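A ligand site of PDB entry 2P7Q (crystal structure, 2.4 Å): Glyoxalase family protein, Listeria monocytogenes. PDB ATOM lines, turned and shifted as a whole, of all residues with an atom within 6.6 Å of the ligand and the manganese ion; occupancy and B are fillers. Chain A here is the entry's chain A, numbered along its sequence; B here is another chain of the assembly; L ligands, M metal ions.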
ATOM      1  N   TYR A  67      -4.307  22.689 -18.930  1.00  0.00           N
ATOM      2  CA  TYR A  67      -3.169  22.750 -18.041  1.00  0.00           C
ATOM      3  C   TYR A  67      -2.818  24.171 -17.670  1.00  0.00           C
ATOM      4  O   TYR A  67      -1.868  24.412 -16.945  1.00  0.00           O
ATOM      5  CB  TYR A  67      -1.960  22.052 -18.653  1.00  0.00           C
ATOM      6  CG  TYR A  67      -0.818  21.847 -17.680  1.00  0.00           C
ATOM      7  CD1 TYR A  67      -1.045  21.313 -16.412  1.00  0.00           C
ATOM      8  CD2 TYR A  67       0.488  22.208 -18.025  1.00  0.00           C
ATOM      9  CE1 TYR A  67       0.010  21.152 -15.501  1.00  0.00           C
ATOM     10  CE2 TYR A  67       1.546  22.056 -17.119  1.00  0.00           C
ATOM     11  CZ  TYR A  67       1.302  21.530 -15.867  1.00  0.00           C
ATOM     12  OH  TYR A  67       2.338  21.408 -14.964  1.00  0.00           O
ATOM     13  N   HIS A  69      -2.738  27.110 -15.506  1.00  0.00           N
ATOM     14  CA  HIS A  69      -2.967  27.174 -14.066  1.00  0.00           C
ATOM     15  C   HIS A  69      -2.277  28.328 -13.353  1.00  0.00           C
ATOM     16  O   HIS A  69      -1.382  28.987 -13.878  1.00  0.00           O
ATOM     17  CB  HIS A  69      -2.556  25.849 -13.382  1.00  0.00           C
ATOM     18  CG  HIS A  69      -1.110  25.477 -13.556  1.00  0.00           C
ATOM     19  ND1 HIS A  69      -0.660  24.755 -14.635  1.00  0.00           N
ATOM     20  CD2 HIS A  69      -0.034  25.686 -12.763  1.00  0.00           C
ATOM     21  CE1 HIS A  69       0.637  24.533 -14.502  1.00  0.00           C
ATOM     22  NE2 HIS A  69       1.039  25.085 -13.375  1.00  0.00           N
ATOM     23  N   ILE A  70      -2.740  28.570 -12.130  1.00  0.00           N
ATOM     24  CA  ILE A  70      -2.191  29.612 -11.278  1.00  0.00           C
ATOM     25  C   ILE A  70      -1.541  28.822 -10.164  1.00  0.00           C
ATOM     26  O   ILE A  70      -2.064  27.792  -9.746  1.00  0.00           O
ATOM     27  CB  ILE A  70      -3.302  30.498 -10.716  1.00  0.00           C
ATOM     28  CG1 ILE A  70      -4.199  30.975 -11.863  1.00  0.00           C
ATOM     29  CG2 ILE A  70      -2.716  31.706 -10.016  1.00  0.00           C
ATOM     30  CD1 ILE A  70      -5.289  31.932 -11.441  1.00  0.00           C
ATOM     31  N   ALA A  71      -0.390  29.266  -9.701  1.00  0.00           N
ATOM     32  CA  ALA A  71       0.329  28.527  -8.668  1.00  0.00           C
ATOM     33  C   ALA A  71       0.729  29.406  -7.513  1.00  0.00           C
ATOM     34  O   ALA A  71       1.321  30.464  -7.707  1.00  0.00           O
ATOM     35  CB  ALA A  71       1.556  27.873  -9.254  1.00  0.00           C
ATOM     36  N   ARG A  97       2.580  14.679 -10.351  1.00  0.00           N
ATOM     37  CA  ARG A  97       3.115  14.912 -11.683  1.00  0.00           C
ATOM     38  C   ARG A  97       4.610  14.537 -11.699  1.00  0.00           C
ATOM     39  O   ARG A  97       5.315  14.754 -10.700  1.00  0.00           O
ATOM     40  CB  ARG A  97       2.909  16.380 -12.020  1.00  0.00           C
ATOM     41  CG  ARG A  97       3.029  16.734 -13.467  1.00  0.00           C
ATOM     42  CD  ARG A  97       2.737  18.198 -13.672  1.00  0.00           C
ATOM     43  NE  ARG A  97       2.813  18.568 -15.075  1.00  0.00           N
ATOM     44  CZ  ARG A  97       1.948  18.150 -15.999  1.00  0.00           C
ATOM     45  NH1 ARG A  97       0.951  17.355 -15.655  1.00  0.00           N
ATOM     46  NH2 ARG A  97       2.108  18.521 -17.260  1.00  0.00           N
ATOM     47  N   PRO A  98       5.112  13.981 -12.813  1.00  0.00           N
ATOM     48  CA  PRO A  98       6.537  13.596 -12.915  1.00  0.00           C
ATOM     49  C   PRO A  98       7.489  14.767 -12.694  1.00  0.00           C
ATOM     50  O   PRO A  98       7.380  15.791 -13.359  1.00  0.00           O
ATOM     51  CB  PRO A  98       6.639  13.021 -14.323  1.00  0.00           C
ATOM     52  CG  PRO A  98       5.267  12.470 -14.559  1.00  0.00           C
ATOM     53  CD  PRO A  98       4.379  13.564 -14.020  1.00  0.00           C
ATOM     54  N   ARG A  99       8.429  14.592 -11.755  1.00  0.00           N
ATOM     55  CA  ARG A  99       9.408  15.617 -11.411  1.00  0.00           C
ATOM     56  C   ARG A  99      10.792  15.416 -12.050  1.00  0.00           C
ATOM     57  O   ARG A  99      10.956  14.589 -12.944  1.00  0.00           O
ATOM     58  CB  ARG A  99       9.589  15.678  -9.886  1.00  0.00           C
ATOM     59  CG  ARG A  99       8.496  16.440  -9.149  1.00  0.00           C
ATOM     60  CD  ARG A  99       8.610  16.239  -7.641  1.00  0.00           C
ATOM     61  NE  ARG A  99       8.165  14.914  -7.228  1.00  0.00           N
ATOM     62  CZ  ARG A  99       8.289  14.436  -6.000  1.00  0.00           C
ATOM     63  NH1 ARG A  99       8.851  15.163  -5.058  1.00  0.00           N
ATOM     64  NH2 ARG A  99       7.845  13.205  -5.718  1.00  0.00           N
ATOM     65  N   GLU A 103      13.049  19.527  -8.399  1.00  0.00           N
ATOM     66  CA  GLU A 103      11.788  20.197  -8.671  1.00  0.00           C
ATOM     67  C   GLU A 103      10.958  19.879  -7.423  1.00  0.00           C
ATOM     68  O   GLU A 103      10.683  18.712  -7.134  1.00  0.00           O
ATOM     69  CB  GLU A 103      11.151  19.588  -9.925  1.00  0.00           C
ATOM     70  CG  GLU A 103       9.905  20.280 -10.473  1.00  0.00           C
ATOM     71  CD  GLU A 103       9.447  19.684 -11.804  1.00  0.00           C
ATOM     72  OE1 GLU A 103       8.400  20.108 -12.341  1.00  0.00           O
ATOM     73  OE2 GLU A 103      10.146  18.781 -12.314  1.00  0.00           O
ATOM     74  N   GLY A 104      10.585  20.918  -6.673  1.00  0.00           N
ATOM     75  CA  GLY A 104       9.825  20.711  -5.458  1.00  0.00           C
ATOM     76  C   GLY A 104       8.481  20.029  -5.654  1.00  0.00           C
ATOM     77  O   GLY A 104       7.962  19.976  -6.778  1.00  0.00           O
ATOM     78  N   SER A 106       4.430  19.369  -5.588  1.00  0.00           N
ATOM     79  CA  SER A 106       3.287  20.219  -5.936  1.00  0.00           C
ATOM     80  C   SER A 106       1.960  19.500  -5.669  1.00  0.00           C
ATOM     81  O   SER A 106       1.899  18.273  -5.632  1.00  0.00           O
ATOM     82  CB  SER A 106       3.324  20.597  -7.415  1.00  0.00           C
ATOM     83  OG  SER A 106       4.429  21.420  -7.747  1.00  0.00           O
ATOM     84  N   TYR A 108      -1.968  19.676  -7.171  1.00  0.00           N
ATOM     85  CA  TYR A 108      -2.840  20.253  -8.184  1.00  0.00           C
ATOM     86  C   TYR A 108      -4.278  19.886  -7.851  1.00  0.00           C
ATOM     87  O   TYR A 108      -4.532  18.806  -7.304  1.00  0.00           O
ATOM     88  CB  TYR A 108      -2.468  19.730  -9.582  1.00  0.00           C
ATOM     89  CG  TYR A 108      -1.296  20.465 -10.225  1.00  0.00           C
ATOM     90  CD1 TYR A 108      -0.007  19.917 -10.255  1.00  0.00           C
ATOM     91  CD2 TYR A 108      -1.497  21.705 -10.840  1.00  0.00           C
ATOM     92  CE1 TYR A 108       1.045  20.590 -10.892  1.00  0.00           C
ATOM     93  CE2 TYR A 108      -0.445  22.378 -11.478  1.00  0.00           C
ATOM     94  CZ  TYR A 108       0.817  21.821 -11.497  1.00  0.00           C
ATOM     95  OH  TYR A 108       1.829  22.503 -12.144  1.00  0.00           O
ATOM     96  N   GLU A 118      -2.727  25.250  -8.038  1.00  0.00           N
ATOM     97  CA  GLU A 118      -1.561  24.521  -7.586  1.00  0.00           C
ATOM     98  C   GLU A 118      -0.911  25.186  -6.396  1.00  0.00           C
ATOM     99  O   GLU A 118      -0.828  26.408  -6.320  1.00  0.00           O
ATOM    100  CB  GLU A 118      -0.525  24.396  -8.701  1.00  0.00           C
ATOM    101  CG  GLU A 118       0.884  24.070  -8.186  1.00  0.00           C
ATOM    102  CD  GLU A 118       1.919  24.042  -9.301  1.00  0.00           C
ATOM    103  OE1 GLU A 118       1.748  24.816 -10.264  1.00  0.00           O
ATOM    104  OE2 GLU A 118       2.898  23.267  -9.184  1.00  0.00           O
ATOM    105  N   HIS A 120       2.588  25.105  -4.912  1.00  0.00           N
ATOM    106  CA  HIS A 120       3.953  24.688  -5.217  1.00  0.00           C
ATOM    107  C   HIS A 120       4.932  24.903  -4.067  1.00  0.00           C
ATOM    108  O   HIS A 120       4.956  25.952  -3.432  1.00  0.00           O
ATOM    109  CB  HIS A 120       4.441  25.452  -6.466  1.00  0.00           C
ATOM    110  CG  HIS A 120       5.799  25.029  -6.959  1.00  0.00           C
ATOM    111  ND1 HIS A 120       6.087  23.738  -7.354  1.00  0.00           N
ATOM    112  CD2 HIS A 120       6.922  25.749  -7.185  1.00  0.00           C
ATOM    113  CE1 HIS A 120       7.328  23.680  -7.806  1.00  0.00           C
ATOM    114  NE2 HIS A 120       7.857  24.887  -7.708  1.00  0.00           N
ATOM    115  N   ARG A 127      15.159  25.477  -9.828  1.00  0.00           N
ATOM    116  CA  ARG A 127      14.722  25.022 -11.150  1.00  0.00           C
ATOM    117  C   ARG A 127      15.586  25.600 -12.275  1.00  0.00           C
ATOM    118  O   ARG A 127      15.370  25.304 -13.449  1.00  0.00           O
ATOM    119  CB  ARG A 127      13.260  25.434 -11.349  1.00  0.00           C
ATOM    120  CG  ARG A 127      12.598  24.935 -12.614  1.00  0.00           C
ATOM    121  CD  ARG A 127      12.537  23.416 -12.651  1.00  0.00           C
ATOM    122  NE  ARG A 127      11.549  22.956 -13.623  1.00  0.00           N
ATOM    123  CZ  ARG A 127      10.234  23.044 -13.447  1.00  0.00           C
ATOM    124  NH1 ARG A 127       9.738  23.564 -12.327  1.00  0.00           N
ATOM    125  NH2 ARG A 127       9.410  22.609 -14.397  1.00  0.00           N
ATOM    126  N   HIS B   7       3.784  31.216  -9.586  1.00  0.00           N
ATOM    127  CA  HIS B   7       3.855  31.427 -11.019  1.00  0.00           C
ATOM    128  C   HIS B   7       2.542  31.140 -11.737  1.00  0.00           C
ATOM    129  O   HIS B   7       1.633  30.536 -11.164  1.00  0.00           O
ATOM    130  CB  HIS B   7       4.914  30.523 -11.626  1.00  0.00           C
ATOM    131  CG  HIS B   7       4.622  29.065 -11.463  1.00  0.00           C
ATOM    132  ND1 HIS B   7       5.051  28.335 -10.363  1.00  0.00           N
ATOM    133  CD2 HIS B   7       3.929  28.200 -12.240  1.00  0.00           C
ATOM    134  CE1 HIS B   7       4.638  27.085 -10.487  1.00  0.00           C
ATOM    135  NE2 HIS B   7       3.953  26.983 -11.611  1.00  0.00           N
ATOM    136  N   ILE B   8       2.452  31.570 -12.989  1.00  0.00           N
ATOM    137  CA  ILE B   8       1.270  31.339 -13.823  1.00  0.00           C
ATOM    138  C   ILE B   8       1.737  30.597 -15.079  1.00  0.00           C
ATOM    139  O   ILE B   8       2.671  31.029 -15.752  1.00  0.00           O
ATOM    140  CB  ILE B   8       0.611  32.654 -14.273  1.00  0.00           C
ATOM    141  CG1 ILE B   8       0.190  33.484 -13.065  1.00  0.00           C
ATOM    142  CG2 ILE B   8      -0.566  32.356 -15.183  1.00  0.00           C
ATOM    143  CD1 ILE B   8      -0.473  34.792 -13.445  1.00  0.00           C
ATOM    144  N   THR B   9       1.083  29.479 -15.402  1.00  0.00           N
ATOM    145  CA  THR B   9       1.441  28.703 -16.576  1.00  0.00           C
ATOM    146  C   THR B   9       0.361  28.769 -17.649  1.00  0.00           C
ATOM    147  O   THR B   9      -0.801  28.492 -17.386  1.00  0.00           O
ATOM    148  CB  THR B   9       1.680  27.240 -16.187  1.00  0.00           C
ATOM    149  OG1 THR B   9       2.884  27.148 -15.424  1.00  0.00           O
ATOM    150  CG2 THR B   9       1.785  26.363 -17.423  1.00  0.00           C
ATOM    151  N   GLU B  44       8.908  24.255 -23.328  1.00  0.00           N
ATOM    152  CA  GLU B  44       8.461  25.236 -22.362  1.00  0.00           C
ATOM    153  C   GLU B  44       9.488  26.334 -22.204  1.00  0.00           C
ATOM    154  O   GLU B  44      10.641  26.188 -22.589  1.00  0.00           O
ATOM    155  CB  GLU B  44       8.185  24.575 -21.008  1.00  0.00           C
ATOM    156  CG  GLU B  44       9.251  23.597 -20.551  1.00  0.00           C
ATOM    157  CD  GLU B  44       8.863  22.912 -19.247  1.00  0.00           C
ATOM    158  OE1 GLU B  44       9.589  21.977 -18.824  1.00  0.00           O
ATOM    159  OE2 GLU B  44       7.847  23.317 -18.651  1.00  0.00           O
ATOM    160  N   PHE B  46      10.408  29.972 -19.511  1.00  0.00           N
ATOM    161  CA  PHE B  46      10.082  30.701 -18.296  1.00  0.00           C
ATOM    162  C   PHE B  46      10.513  32.129 -18.508  1.00  0.00           C
ATOM    163  O   PHE B  46      11.670  32.373 -18.835  1.00  0.00           O
ATOM    164  CB  PHE B  46      10.849  30.153 -17.081  1.00  0.00           C
ATOM    165  CG  PHE B  46      10.544  28.724 -16.722  1.00  0.00           C
ATOM    166  CD1 PHE B  46      11.268  28.090 -15.734  1.00  0.00           C
ATOM    167  CD2 PHE B  46       9.531  28.009 -17.371  1.00  0.00           C
ATOM    168  CE1 PHE B  46      10.998  26.777 -15.381  1.00  0.00           C
ATOM    169  CE2 PHE B  46       9.254  26.694 -17.026  1.00  0.00           C
ATOM    170  CZ  PHE B  46       9.993  26.073 -16.027  1.00  0.00           C
ATOM    171  N   TRP B  53       7.141  35.249 -12.120  1.00  0.00           N
ATOM    172  CA  TRP B  53       7.534  34.075 -12.862  1.00  0.00           C
ATOM    173  C   TRP B  53       6.396  33.553 -13.741  1.00  0.00           C
ATOM    174  O   TRP B  53       5.385  33.077 -13.241  1.00  0.00           O
ATOM    175  CB  TRP B  53       7.981  32.984 -11.884  1.00  0.00           C
ATOM    176  CG  TRP B  53       8.257  31.640 -12.514  1.00  0.00           C
ATOM    177  CD1 TRP B  53       8.386  31.365 -13.858  1.00  0.00           C
ATOM    178  CD2 TRP B  53       8.440  30.395 -11.832  1.00  0.00           C
ATOM    179  NE1 TRP B  53       8.649  30.033 -14.041  1.00  0.00           N
ATOM    180  CE2 TRP B  53       8.687  29.407 -12.810  1.00  0.00           C
ATOM    181  CE3 TRP B  53       8.430  30.015 -10.490  1.00  0.00           C
ATOM    182  CZ2 TRP B  53       8.910  28.071 -12.483  1.00  0.00           C
ATOM    183  CZ3 TRP B  53       8.653  28.680 -10.163  1.00  0.00           C
ATOM    184  CH2 TRP B  53       8.891  27.733 -11.158  1.00  0.00           C
ATOM    185  N   CYS B  55       5.359  30.918 -16.815  1.00  0.00           N
ATOM    186  CA  CYS B  55       5.724  29.735 -17.572  1.00  0.00           C
ATOM    187  C   CYS B  55       4.807  29.540 -18.776  1.00  0.00           C
ATOM    188  O   CYS B  55       3.579  29.559 -18.647  1.00  0.00           O
ATOM    189  CB  CYS B  55       5.686  28.510 -16.673  1.00  0.00           C
ATOM    190  SG  CYS B  55       5.710  26.928 -17.547  1.00  0.00           S
ATOM    191  N   MET B  57       3.934  26.952 -21.900  1.00  0.00           N
ATOM    192  CA  MET B  57       4.137  25.586 -22.377  1.00  0.00           C
ATOM    193  C   MET B  57       3.377  25.412 -23.682  1.00  0.00           C
ATOM    194  O   MET B  57       2.360  26.053 -23.915  1.00  0.00           O
ATOM    195  CB  MET B  57       3.661  24.576 -21.328  1.00  0.00           C
ATOM    196  CG  MET B  57       4.147  23.160 -21.583  1.00  0.00           C
ATOM    197  SD  MET B  57       3.556  21.967 -20.356  1.00  0.00           S
ATOM    198  CE  MET B  57       4.707  22.249 -19.059  1.00  0.00           C
HETATM  199  O1  LIG L   1       4.390  23.328 -11.596  1.00  0.00           O
HETATM  200  C1  LIG L   1       5.788  23.263 -12.024  1.00  0.00           C
HETATM  201  C2  LIG L   1       6.535  22.179 -11.163  1.00  0.00           C
HETATM  202  C3  LIG L   1       5.891  22.894 -13.555  1.00  0.00           C
HETATM  203  O2  LIG L   1       5.327  21.613 -13.812  1.00  0.00           O
HETATM  204  P1  LIG L   1       5.077  24.063 -14.608  1.00  0.00           P
HETATM  205  O3  LIG L   1       5.683  25.484 -14.396  1.00  0.00           O
HETATM  206  O4  LIG L   1       5.260  23.642 -15.965  1.00  0.00           O
HETATM  207  O5  LIG L   1       3.520  24.125 -14.288  1.00  0.00           O
HETATM  208 MN    MN M   1       3.108  24.871 -12.275  1.00  0.00          MN
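The side-chain hydroxyl (OH) of Tyr 67 lies within hydrogen-bond range of an oxygen (O2) of the ligand (3.2 Å). The side-chain hydroxyl of Thr 9 of chain B is in hydrogen-bond range of an oxygen (O3) of the ligand (3.4 Å). An oxygen (O3) of the ligand lies within hydrogen-bond range of the side-chain sulfur of Cys 55 of chain B (3.5 Å).
Glu 103 touches the ligand. His 120 touches the ligand (CE1 to C2, 3.8 Å). Arg 127 touches the ligand. Glu 44 of chain B touches the ligand (OE2 to O4, 3.7 Å). CE of Met 57 of chain B touches O4 of the ligand (3.4 Å). Hydrophobic or aromatic side chains within 4 Å of the ligand: Tyr 67, His 69, Tyr 108, His 120, His 7 of chain B and Met 57 of chain B. Of the 22 residues printed, 12 come within 4 Å of the ligand.
An oxygen (O1) of the ligand binds the manganese ion, at 2.1 Å. O5 of the ligand is bound to the manganese ion, at 2.2 Å. The manganese ion is bound by NE2 of His 69, 2.4 Å away. A ring nitrogen (NE2) of His 7 of chain B binds the manganese ion, 2.4 Å away. OE1 of Glu 118 is bound to the manganese ion (2.4 Å). The manganese ion is bound by the side-chain hydroxyl (OH) of Tyr 108, 2.7 Å away. The manganese ion has six donor atoms within binding distance.
O of Tyr 67 is in hydrogen-bond range of ND1 of His 69, at 2.6 Å. O of His 69 lies within hydrogen-bond range of N of Thr 9 of chain B. The backbone NH (N) of Ala 71 is in hydrogen-bond range of the backbone carbonyl oxygen (O) of His 7 of chain B. The side-chain hydroxyl of Tyr 67 sits close to the side-chain hydroxyl of Tyr 108 (3.1 Å). OE1 of Glu 103 lies within salt-bridge range of NH2 of Arg 127 (3.4 Å). The side-chain hydroxyl (OH) of Tyr 67 is in hydrogen-bond range of the guanidinium group (NE) of Arg 97, 2.9 Å away. OG1 of Thr 9 of chain B lies close to SG of Cys 55 of chain B (3.5 Å). O of Ile 8 of chain B lies within hydrogen-bond range of N of Cys 55 of chain B, at 2.9 Å.
Residues that only touch the manganese ion: Thr 9 of chain B (3.9 Å). Five residues have an atom within 4 Å of the manganese ion: His 69, Tyr 108, Glu 118, His 7 of chain B and Thr 9 of chain B.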
